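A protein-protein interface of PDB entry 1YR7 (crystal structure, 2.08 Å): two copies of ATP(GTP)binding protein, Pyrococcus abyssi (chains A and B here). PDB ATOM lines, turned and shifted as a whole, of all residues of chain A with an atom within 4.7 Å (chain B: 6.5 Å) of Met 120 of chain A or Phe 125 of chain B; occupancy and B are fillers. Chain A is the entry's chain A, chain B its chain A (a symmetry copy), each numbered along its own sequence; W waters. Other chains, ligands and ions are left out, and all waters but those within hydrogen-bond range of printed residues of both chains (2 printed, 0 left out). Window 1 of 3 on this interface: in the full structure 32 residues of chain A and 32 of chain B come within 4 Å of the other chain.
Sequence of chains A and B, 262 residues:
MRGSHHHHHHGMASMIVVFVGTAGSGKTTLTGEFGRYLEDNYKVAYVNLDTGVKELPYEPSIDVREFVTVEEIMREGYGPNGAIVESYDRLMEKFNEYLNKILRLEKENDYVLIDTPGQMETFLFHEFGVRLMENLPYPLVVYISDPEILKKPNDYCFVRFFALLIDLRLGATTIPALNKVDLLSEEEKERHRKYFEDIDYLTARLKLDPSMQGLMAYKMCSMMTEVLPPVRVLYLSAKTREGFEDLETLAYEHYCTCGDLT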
ATOM      1  N   VAL A  20      13.725  22.041   8.527  1.00  0.00           N
ATOM      2  CA  VAL A  20      13.472  20.606   8.431  1.00  0.00           C
ATOM      3  C   VAL A  20      12.138  20.271   9.124  1.00  0.00           C
ATOM      4  O   VAL A  20      11.856  20.783  10.193  1.00  0.00           O
ATOM      5  CB  VAL A  20      14.613  19.796   9.082  1.00  0.00           C
ATOM      6  CG1 VAL A  20      14.231  18.352   9.215  1.00  0.00           C
ATOM      7  CG2 VAL A  20      15.889  19.914   8.230  1.00  0.00           C
ATOM      8  N   GLY A  21      11.317  19.447   8.491  1.00  0.00           N
ATOM      9  CA  GLY A  21       9.978  19.235   8.962  1.00  0.00           C
ATOM     10  C   GLY A  21       9.215  18.377   7.988  1.00  0.00           C
ATOM     11  O   GLY A  21       9.604  18.224   6.819  1.00  0.00           O
ATOM     12  N   THR A  22       8.111  17.815   8.470  1.00  0.00           N
ATOM     13  CA  THR A  22       7.305  16.975   7.641  1.00  0.00           C
ATOM     14  C   THR A  22       6.608  17.863   6.588  1.00  0.00           C
ATOM     15  O   THR A  22       6.440  19.083   6.791  1.00  0.00           O
ATOM     16  CB  THR A  22       6.324  16.143   8.510  1.00  0.00           C
ATOM     17  OG1 THR A  22       6.066  14.893   7.869  1.00  0.00           O
ATOM     18  CG2 THR A  22       5.048  16.893   8.755  1.00  0.00           C
ATOM     19  N   PRO A 117      13.824  19.122   1.106  1.00  0.00           N
ATOM     20  CA  PRO A 117      12.838  18.265   0.450  1.00  0.00           C
ATOM     21  C   PRO A 117      11.522  18.241   1.220  1.00  0.00           C
ATOM     22  O   PRO A 117      11.520  18.149   2.444  1.00  0.00           O
ATOM     23  CB  PRO A 117      13.479  16.884   0.506  1.00  0.00           C
ATOM     24  CG  PRO A 117      14.933  17.120   0.573  1.00  0.00           C
ATOM     25  CD  PRO A 117      15.152  18.492   1.177  1.00  0.00           C
ATOM     26  N   GLY A 118      10.417  18.357   0.499  1.00  0.00           N
ATOM     27  CA  GLY A 118       9.104  18.173   1.073  1.00  0.00           C
ATOM     28  C   GLY A 118       9.015  17.147   2.187  1.00  0.00           C
ATOM     29  O   GLY A 118       8.436  17.446   3.233  1.00  0.00           O
ATOM     30  N   GLN A 119       9.554  15.946   1.958  1.00  0.00           N
ATOM     31  CA  GLN A 119       9.568  14.885   2.972  1.00  0.00           C
ATOM     32  C   GLN A 119      10.893  14.911   3.710  1.00  0.00           C
ATOM     33  O   GLN A 119      11.936  14.831   3.102  1.00  0.00           O
ATOM     34  CB  GLN A 119       9.387  13.480   2.348  1.00  0.00           C
ATOM     35  CG  GLN A 119       8.296  13.350   1.248  1.00  0.00           C
ATOM     36  CD  GLN A 119       6.898  13.154   1.802  1.00  0.00           C
ATOM     37  OE1 GLN A 119       6.704  12.528   2.845  1.00  0.00           O
ATOM     38  NE2 GLN A 119       5.909  13.694   1.102  1.00  0.00           N
ATOM     39  N   MET A 120      10.874  14.988   5.022  1.00  0.00           N
ATOM     40  CA  MET A 120      12.172  15.093   5.688  1.00  0.00           C
ATOM     41  C   MET A 120      12.986  13.811   5.611  1.00  0.00           C
ATOM     42  O   MET A 120      14.209  13.851   5.672  1.00  0.00           O
ATOM     43  CB  MET A 120      12.059  15.639   7.104  1.00  0.00           C
ATOM     44  CG  MET A 120      11.302  14.776   8.019  1.00  0.00           C
ATOM     45  SD  MET A 120      11.187  15.493   9.651  1.00  0.00           S
ATOM     46  CE  MET A 120      10.041  14.270  10.311  1.00  0.00           C
ATOM     47  N   GLU A 121      12.325  12.678   5.396  1.00  0.00           N
ATOM     48  CA  GLU A 121      13.066  11.416   5.245  1.00  0.00           C
ATOM     49  C   GLU A 121      13.888  11.366   3.977  1.00  0.00           C
ATOM     50  O   GLU A 121      14.891  10.671   3.903  1.00  0.00           O
ATOM     51  CB  GLU A 121      12.169  10.172   5.389  1.00  0.00           C
ATOM     52  CG  GLU A 121      11.298   9.832   4.202  1.00  0.00           C
ATOM     53  CD  GLU A 121      10.194   8.864   4.601  1.00  0.00           C
ATOM     54  OE1 GLU A 121      10.316   7.654   4.318  1.00  0.00           O
ATOM     55  OE2 GLU A 121       9.213   9.324   5.226  1.00  0.00           O
ATOM     56  N   THR A 122      13.484  12.129   2.972  1.00  0.00           N
ATOM     57  CA  THR A 122      14.334  12.260   1.813  1.00  0.00           C
ATOM     58  C   THR A 122      15.651  12.895   2.237  1.00  0.00           C
ATOM     59  O   THR A 122      16.705  12.460   1.791  1.00  0.00           O
ATOM     60  CB  THR A 122      13.682  13.087   0.733  1.00  0.00           C
ATOM     61  OG1 THR A 122      12.510  12.406   0.279  1.00  0.00           O
ATOM     62  CG2 THR A 122      14.633  13.276  -0.430  1.00  0.00           C
ATOM     63  N   PHE A 123      15.586  13.890   3.128  1.00  0.00           N
ATOM     64  CA  PHE A 123      16.784  14.586   3.619  1.00  0.00           C
ATOM     65  C   PHE A 123      17.580  13.721   4.583  1.00  0.00           C
ATOM     66  O   PHE A 123      18.828  13.680   4.535  1.00  0.00           O
ATOM     67  CB  PHE A 123      16.398  15.931   4.312  1.00  0.00           C
ATOM     68  CG  PHE A 123      17.535  16.927   4.391  1.00  0.00           C
ATOM     69  CD1 PHE A 123      18.179  17.370   3.217  1.00  0.00           C
ATOM     70  CD2 PHE A 123      17.953  17.435   5.618  1.00  0.00           C
ATOM     71  CE1 PHE A 123      19.257  18.274   3.288  1.00  0.00           C
ATOM     72  CE2 PHE A 123      18.987  18.336   5.690  1.00  0.00           C
ATOM     73  CZ  PHE A 123      19.658  18.750   4.527  1.00  0.00           C
ATOM     74  N   LEU A 124      16.865  13.052   5.489  1.00  0.00           N
ATOM     75  CA  LEU A 124      17.501  12.354   6.597  1.00  0.00           C
ATOM     76  C   LEU A 124      18.060  10.996   6.190  1.00  0.00           C
ATOM     77  O   LEU A 124      19.020  10.517   6.769  1.00  0.00           O
ATOM     78  CB  LEU A 124      16.519  12.194   7.767  1.00  0.00           C
ATOM     79  CG  LEU A 124      16.124  13.491   8.478  1.00  0.00           C
ATOM     80  CD1 LEU A 124      15.171  13.190   9.595  1.00  0.00           C
ATOM     81  CD2 LEU A 124      17.379  14.225   9.032  1.00  0.00           C
ATOM     82  N   TYR A 143      13.953  22.368  13.344  1.00  0.00           N
ATOM     83  CA  TYR A 143      12.997  21.290  13.099  1.00  0.00           C
ATOM     84  C   TYR A 143      11.632  21.744  13.552  1.00  0.00           C
ATOM     85  O   TYR A 143      11.444  22.006  14.731  1.00  0.00           O
ATOM     86  CB  TYR A 143      13.422  20.054  13.896  1.00  0.00           C
ATOM     87  CG  TYR A 143      12.338  19.020  14.143  1.00  0.00           C
ATOM     88  CD1 TYR A 143      11.606  18.440  13.099  1.00  0.00           C
ATOM     89  CD2 TYR A 143      12.112  18.558  15.421  1.00  0.00           C
ATOM     90  CE1 TYR A 143      10.619  17.467  13.372  1.00  0.00           C
ATOM     91  CE2 TYR A 143      11.141  17.604  15.697  1.00  0.00           C
ATOM     92  CZ  TYR A 143      10.409  17.064  14.686  1.00  0.00           C
ATOM     93  OH  TYR A 143       9.490  16.091  15.051  1.00  0.00           O
ATOM     94  N   ILE A 149      -0.059  17.813  15.413  1.00  0.00           N
ATOM     95  CA  ILE A 149       0.432  16.497  15.796  1.00  0.00           C
ATOM     96  C   ILE A 149       0.355  16.295  17.302  1.00  0.00           C
ATOM     97  O   ILE A 149       0.545  15.185  17.791  1.00  0.00           O
ATOM     98  CB  ILE A 149       1.912  16.267  15.384  1.00  0.00           C
ATOM     99  CG1 ILE A 149       2.853  17.093  16.274  1.00  0.00           C
ATOM    100  CG2 ILE A 149       2.120  16.539  13.890  1.00  0.00           C
ATOM    101  CD1 ILE A 149       4.202  16.439  16.491  1.00  0.00           C
ATOM    102  N   PHE A 158       7.985  13.074  21.936  1.00  0.00           N
ATOM    103  CA  PHE A 158       8.283  12.680  20.577  1.00  0.00           C
ATOM    104  C   PHE A 158       8.985  13.816  19.818  1.00  0.00           C
ATOM    105  O   PHE A 158      10.098  13.647  19.341  1.00  0.00           O
ATOM    106  CB  PHE A 158       6.972  12.272  19.917  1.00  0.00           C
ATOM    107  CG  PHE A 158       7.031  12.178  18.430  1.00  0.00           C
ATOM    108  CD1 PHE A 158       7.822  11.220  17.810  1.00  0.00           C
ATOM    109  CD2 PHE A 158       6.251  13.013  17.648  1.00  0.00           C
ATOM    110  CE1 PHE A 158       7.858  11.118  16.431  1.00  0.00           C
ATOM    111  CE2 PHE A 158       6.279  12.919  16.274  1.00  0.00           C
ATOM    112  CZ  PHE A 158       7.088  11.970  15.663  1.00  0.00           C
ATOM    113  N   PHE A 162      12.696  13.544  18.446  1.00  0.00           N
ATOM    114  CA  PHE A 162      12.936  13.599  17.016  1.00  0.00           C
ATOM    115  C   PHE A 162      14.056  14.604  16.692  1.00  0.00           C
ATOM    116  O   PHE A 162      14.948  14.292  15.912  1.00  0.00           O
ATOM    117  CB  PHE A 162      11.652  13.823  16.210  1.00  0.00           C
ATOM    118  CG  PHE A 162      11.752  13.344  14.786  1.00  0.00           C
ATOM    119  CD1 PHE A 162      11.406  12.060  14.449  1.00  0.00           C
ATOM    120  CD2 PHE A 162      12.244  14.168  13.792  1.00  0.00           C
ATOM    121  CE1 PHE A 162      11.527  11.601  13.150  1.00  0.00           C
ATOM    122  CE2 PHE A 162      12.365  13.721  12.478  1.00  0.00           C
ATOM    123  CZ  PHE A 162      12.009  12.431  12.160  1.00  0.00           C
ATOM    124  N   ILE A 166      17.463  13.881  14.622  1.00  0.00           N
ATOM    125  CA  ILE A 166      17.900  14.648  13.468  1.00  0.00           C
ATOM    126  C   ILE A 166      19.309  15.119  13.755  1.00  0.00           C
ATOM    127  O   ILE A 166      20.212  15.043  12.911  1.00  0.00           O
ATOM    128  CB  ILE A 166      16.948  15.855  13.228  1.00  0.00           C
ATOM    129  CG1 ILE A 166      15.588  15.372  12.692  1.00  0.00           C
ATOM    130  CG2 ILE A 166      17.566  16.850  12.282  1.00  0.00           C
ATOM    131  CD1 ILE A 166      14.462  16.380  12.871  1.00  0.00           C
ATOM    132  N   GLN B 119       6.425   6.497   2.157  1.00  0.00           N
ATOM    133  CA  GLN B 119       7.190   7.341   3.083  1.00  0.00           C
ATOM    134  C   GLN B 119       6.731   7.073   4.503  1.00  0.00           C
ATOM    135  O   GLN B 119       5.565   7.188   4.805  1.00  0.00           O
ATOM    136  CB  GLN B 119       7.001   8.848   2.788  1.00  0.00           C
ATOM    137  CG  GLN B 119       7.050   9.268   1.291  1.00  0.00           C
ATOM    138  CD  GLN B 119       8.459   9.462   0.762  1.00  0.00           C
ATOM    139  OE1 GLN B 119       9.361   9.891   1.484  1.00  0.00           O
ATOM    140  NE2 GLN B 119       8.657   9.142  -0.510  1.00  0.00           N
ATOM    141  N   MET B 120       7.636   6.750   5.400  1.00  0.00           N
ATOM    142  CA  MET B 120       7.142   6.421   6.737  1.00  0.00           C
ATOM    143  C   MET B 120       6.597   7.628   7.484  1.00  0.00           C
ATOM    144  O   MET B 120       5.747   7.483   8.355  1.00  0.00           O
ATOM    145  CB  MET B 120       8.150   5.626   7.553  1.00  0.00           C
ATOM    146  CG  MET B 120       9.391   6.354   7.844  1.00  0.00           C
ATOM    147  SD  MET B 120      10.536   5.349   8.778  1.00  0.00           S
ATOM    148  CE  MET B 120      11.913   6.508   8.693  1.00  0.00           C
ATOM    149  N   GLU B 121       7.015   8.828   7.096  1.00  0.00           N
ATOM    150  CA  GLU B 121       6.471  10.036   7.737  1.00  0.00           C
ATOM    151  C   GLU B 121       5.011  10.263   7.415  1.00  0.00           C
ATOM    152  O   GLU B 121       4.286  10.881   8.182  1.00  0.00           O
ATOM    153  CB  GLU B 121       7.316  11.294   7.462  1.00  0.00           C
ATOM    154  CG  GLU B 121       7.162  11.920   6.095  1.00  0.00           C
ATOM    155  CD  GLU B 121       8.309  12.875   5.806  1.00  0.00           C
ATOM    156  OE1 GLU B 121       8.120  14.104   5.921  1.00  0.00           O
ATOM    157  OE2 GLU B 121       9.414  12.381   5.488  1.00  0.00           O
ATOM    158  N   THR B 122       4.559   9.739   6.286  1.00  0.00           N
ATOM    159  CA  THR B 122       3.140   9.767   6.025  1.00  0.00           C
ATOM    160  C   THR B 122       2.425   8.964   7.104  1.00  0.00           C
ATOM    161  O   THR B 122       1.388   9.393   7.594  1.00  0.00           O
ATOM    162  CB  THR B 122       2.811   9.212   4.661  1.00  0.00           C
ATOM    163  OG1 THR B 122       3.403  10.056   3.670  1.00  0.00           O
ATOM    164  CG2 THR B 122       1.312   9.176   4.457  1.00  0.00           C
ATOM    165  N   PHE B 123       3.005   7.825   7.497  1.00  0.00           N
ATOM    166  CA  PHE B 123       2.419   6.959   8.530  1.00  0.00           C
ATOM    167  C   PHE B 123       2.567   7.561   9.918  1.00  0.00           C
ATOM    168  O   PHE B 123       1.632   7.515  10.745  1.00  0.00           O
ATOM    169  CB  PHE B 123       3.070   5.539   8.499  1.00  0.00           C
ATOM    170  CG  PHE B 123       2.222   4.463   9.141  1.00  0.00           C
ATOM    171  CD1 PHE B 123       0.919   4.204   8.671  1.00  0.00           C
ATOM    172  CD2 PHE B 123       2.720   3.700  10.194  1.00  0.00           C
ATOM    173  CE1 PHE B 123       0.117   3.223   9.286  1.00  0.00           C
ATOM    174  CE2 PHE B 123       1.950   2.726  10.781  1.00  0.00           C
ATOM    175  CZ  PHE B 123       0.636   2.491  10.342  1.00  0.00           C
ATOM    176  N   LEU B 124       3.757   8.097  10.195  1.00  0.00           N
ATOM    177  CA  LEU B 124       4.106   8.520  11.543  1.00  0.00           C
ATOM    178  C   LEU B 124       3.525   9.884  11.898  1.00  0.00           C
ATOM    179  O   LEU B 124       3.261  10.170  13.054  1.00  0.00           O
ATOM    180  CB  LEU B 124       5.630   8.529  11.726  1.00  0.00           C
ATOM    181  CG  LEU B 124       6.304   7.155  11.710  1.00  0.00           C
ATOM    182  CD1 LEU B 124       7.782   7.309  11.902  1.00  0.00           C
ATOM    183  CD2 LEU B 124       5.716   6.235  12.818  1.00  0.00           C
ATOM    184  N   PHE B 125       3.307  10.722  10.894  1.00  0.00           N
ATOM    185  CA  PHE B 125       2.845  12.091  11.142  1.00  0.00           C
ATOM    186  C   PHE B 125       1.401  12.389  10.741  1.00  0.00           C
ATOM    187  O   PHE B 125       0.891  13.464  11.039  1.00  0.00           O
ATOM    188  CB  PHE B 125       3.779  13.083  10.453  1.00  0.00           C
ATOM    189  CG  PHE B 125       5.093  13.223  11.135  1.00  0.00           C
ATOM    190  CD1 PHE B 125       5.227  14.054  12.231  1.00  0.00           C
ATOM    191  CD2 PHE B 125       6.186  12.520  10.704  1.00  0.00           C
ATOM    192  CE1 PHE B 125       6.425  14.173  12.877  1.00  0.00           C
ATOM    193  CE2 PHE B 125       7.381  12.631  11.349  1.00  0.00           C
ATOM    194  CZ  PHE B 125       7.514  13.474  12.429  1.00  0.00           C
ATOM    195  N   HIS B 126       0.754  11.480  10.021  1.00  0.00           N
ATOM    196  CA  HIS B 126      -0.629  11.704   9.641  1.00  0.00           C
ATOM    197  C   HIS B 126      -1.556  10.972  10.619  1.00  0.00           C
ATOM    198  O   HIS B 126      -1.265   9.878  11.096  1.00  0.00           O
ATOM    199  CB  HIS B 126      -0.891  11.258   8.194  1.00  0.00           C
ATOM    200  CG  HIS B 126      -2.060  11.941   7.554  1.00  0.00           C
ATOM    201  ND1 HIS B 126      -3.360  11.518   7.731  1.00  0.00           N
ATOM    202  CD2 HIS B 126      -2.121  13.025   6.744  1.00  0.00           C
ATOM    203  CE1 HIS B 126      -4.174  12.314   7.062  1.00  0.00           C
ATOM    204  NE2 HIS B 126      -3.447  13.232   6.446  1.00  0.00           N
ATOM    205  N   GLU B 127      -2.690  11.594  10.883  1.00  0.00           N
ATOM    206  CA  GLU B 127      -3.680  11.093  11.799  1.00  0.00           C
ATOM    207  C   GLU B 127      -4.202   9.690  11.449  1.00  0.00           C
ATOM    208  O   GLU B 127      -4.522   8.884  12.349  1.00  0.00           O
ATOM    209  CB  GLU B 127      -4.823  12.109  11.835  1.00  0.00           C
ATOM    210  CG  GLU B 127      -6.154  11.532  12.170  1.00  0.00           C
ATOM    211  CD  GLU B 127      -7.196  12.610  12.464  1.00  0.00           C
ATOM    212  OE1 GLU B 127      -7.408  13.493  11.619  1.00  0.00           O
ATOM    213  OE2 GLU B 127      -7.801  12.550  13.540  1.00  0.00           O
ATOM    214  N   PHE B 128      -4.323   9.419  10.147  1.00  0.00           N
ATOM    215  CA  PHE B 128      -4.822   8.122   9.683  1.00  0.00           C
ATOM    216  C   PHE B 128      -4.047   6.961  10.297  1.00  0.00           C
ATOM    217  O   PHE B 128      -4.621   6.114  10.994  1.00  0.00           O
ATOM    218  CB  PHE B 128      -4.803   8.012   8.154  1.00  0.00           C
ATOM    219  CG  PHE B 128      -5.453   6.740   7.627  1.00  0.00           C
ATOM    220  CD1 PHE B 128      -6.840   6.609   7.592  1.00  0.00           C
ATOM    221  CD2 PHE B 128      -4.676   5.678   7.170  1.00  0.00           C
ATOM    222  CE1 PHE B 128      -7.440   5.451   7.117  1.00  0.00           C
ATOM    223  CE2 PHE B 128      -5.263   4.510   6.684  1.00  0.00           C
ATOM    224  CZ  PHE B 128      -6.653   4.395   6.660  1.00  0.00           C
ATOM    225  N   VAL B 130      -1.527   6.961  12.565  1.00  0.00           N
ATOM    226  CA  VAL B 130      -1.401   7.068  14.007  1.00  0.00           C
ATOM    227  C   VAL B 130      -2.656   6.546  14.730  1.00  0.00           C
ATOM    228  O   VAL B 130      -2.547   5.793  15.680  1.00  0.00           O
ATOM    229  CB  VAL B 130      -1.073   8.502  14.428  1.00  0.00           C
ATOM    230  CG1 VAL B 130      -1.207   8.693  15.961  1.00  0.00           C
ATOM    231  CG2 VAL B 130       0.346   8.853  13.986  1.00  0.00           C
ATOM    232  N   ARG B 169       5.832   7.071  19.253  1.00  0.00           N
ATOM    233  CA  ARG B 169       4.828   7.702  18.404  1.00  0.00           C
ATOM    234  C   ARG B 169       3.583   6.851  18.054  1.00  0.00           C
ATOM    235  O   ARG B 169       2.467   7.387  17.983  1.00  0.00           O
ATOM    236  CB  ARG B 169       5.527   8.193  17.133  1.00  0.00           C
ATOM    237  CG  ARG B 169       4.637   8.916  16.138  1.00  0.00           C
ATOM    238  CD  ARG B 169       4.035  10.190  16.730  1.00  0.00           C
ATOM    239  NE  ARG B 169       3.137  10.782  15.761  1.00  0.00           N
ATOM    240  CZ  ARG B 169       2.270  11.750  16.026  1.00  0.00           C
ATOM    241  NH1 ARG B 169       2.167  12.243  17.251  1.00  0.00           N
ATOM    242  NH2 ARG B 169       1.494  12.218  15.052  1.00  0.00           N
HETATM  243  O   HOH W   1       3.884  12.511   4.078  1.00  0.00           O
HETATM  244  O   HOH W   2      12.252   9.888   0.427  1.00  0.00           O
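OE2 of Glu 121 of chain B lies within hydrogen-bond range of N of Glu 121 of chain A (2.9 Å). OG1 of Thr 22 of chain A lies within hydrogen-bond range of OE1 of Glu 121 of chain B. N of Met 120 of chain A is in hydrogen-bond range of OE2 of Glu 121 of chain B, at 3.0 Å. The backbone carbonyl oxygen (O) of Ile 149 of chain A sits at hydrogen-bond distance from the guanidinium group (NH1) of Arg 169 of chain B (3.4 Å). The side-chain carboxylate of Glu 121 of chain A sits at hydrogen-bond distance from the backbone NH of Met 120 of chain B (3.0 Å).
O of Leu 124 of chain B is in hydrogen-bond range of NE of Arg 169 of chain B.
Among the printed residues, merely in contact across the chains: Thr 22 of chain A with Phe 125 of chain B (3.7 Å), Gln 119 of chain A with Gln 119 of chain B (3.6 Å), Gln 119 of chain A with Glu 121 of chain B (3.3 Å), Met 120 of chain A with Phe 125 of chain B (3.3 Å), Glu 121 of chain A with Gln 119 of chain B (3.3 Å), Phe 158 of chain A with Phe 125 of chain B (3.6 Å) and Phe 158 of chain A with Arg 169 of chain B (3.6 Å).
Of chain B, only Glu 121 and Phe 125 come within 4 Å of Met 120 of chain A. Of the printed residues of chain B, Ile 149 of chain A touches Arg 169. Of the printed residues of chain A, Glu 121 of chain B touches Thr 22, Gln 119, Met 120 and Glu 121. Of the printed residues of chain A, Met 120 of chain B touches Glu 121. Printed residues of chain B within 4 Å of Phe 158 of chain A: Phe 125 and Arg 169. Printed residues of chain B within 4 Å of Gln 119 of chain A: Gln 119 and Glu 121. Tyr 143 of chain A touches none of the printed residues of chain B. The nearest residue of chain B that does not touch Met 120 of chain A is Gln 119 of chain B (6.4 Å). The nearest residue of chain A that does not touch Phe 125 of chain B is Tyr 143 of chain A (4.2 Å). The nearest printed residue of chain A that does not touch Arg 169 of chain B is Phe 162 of chain A (7.5 Å).
Of the 16 printed residues of chain A, 6 touch a printed residue of chain B. Of the 12 printed residues of chain B, 5 touch a printed residue of chain A. Printed residues of chain B that touch a printed residue of chain A: Gln 119, Met 120, Glu 121, Phe 125 and Arg 169. Hydrophobic or aromatic side chains of chain B within 4 Å of the printed part of chain A: Met 120 and Phe 125. Among the printed residues, 12 pairs touch across the chains.
Gln 119 of chain B touches its own counterpart, Gln 119 of chain A. Gln 119 of chain A touches Glu 121 of chain B, and with the chains exchanged Glu 121 of chain A touches Gln 119 of chain B. Met 120 of chain A touches Glu 121 of chain B, and with the chains exchanged Glu 121 of chain A touches Met 120 of chain B. Glu 121 of chain A touches its own counterpart, Glu 121 of chain B. Positions printed for both chains: 119, 120, 121, 122, 123 and 124.
Water W2 bridges the side-chain hydroxyl (OG1) of Thr 122 of chain A (2.5 Å) and the side-chain amide oxygen (OE1) of Gln 119 of chain B (3.1 Å). Water W1 lies within hydrogen-bond range of OG1 of Thr 122 of chain B and OE1 of Gln 119 of chain A.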
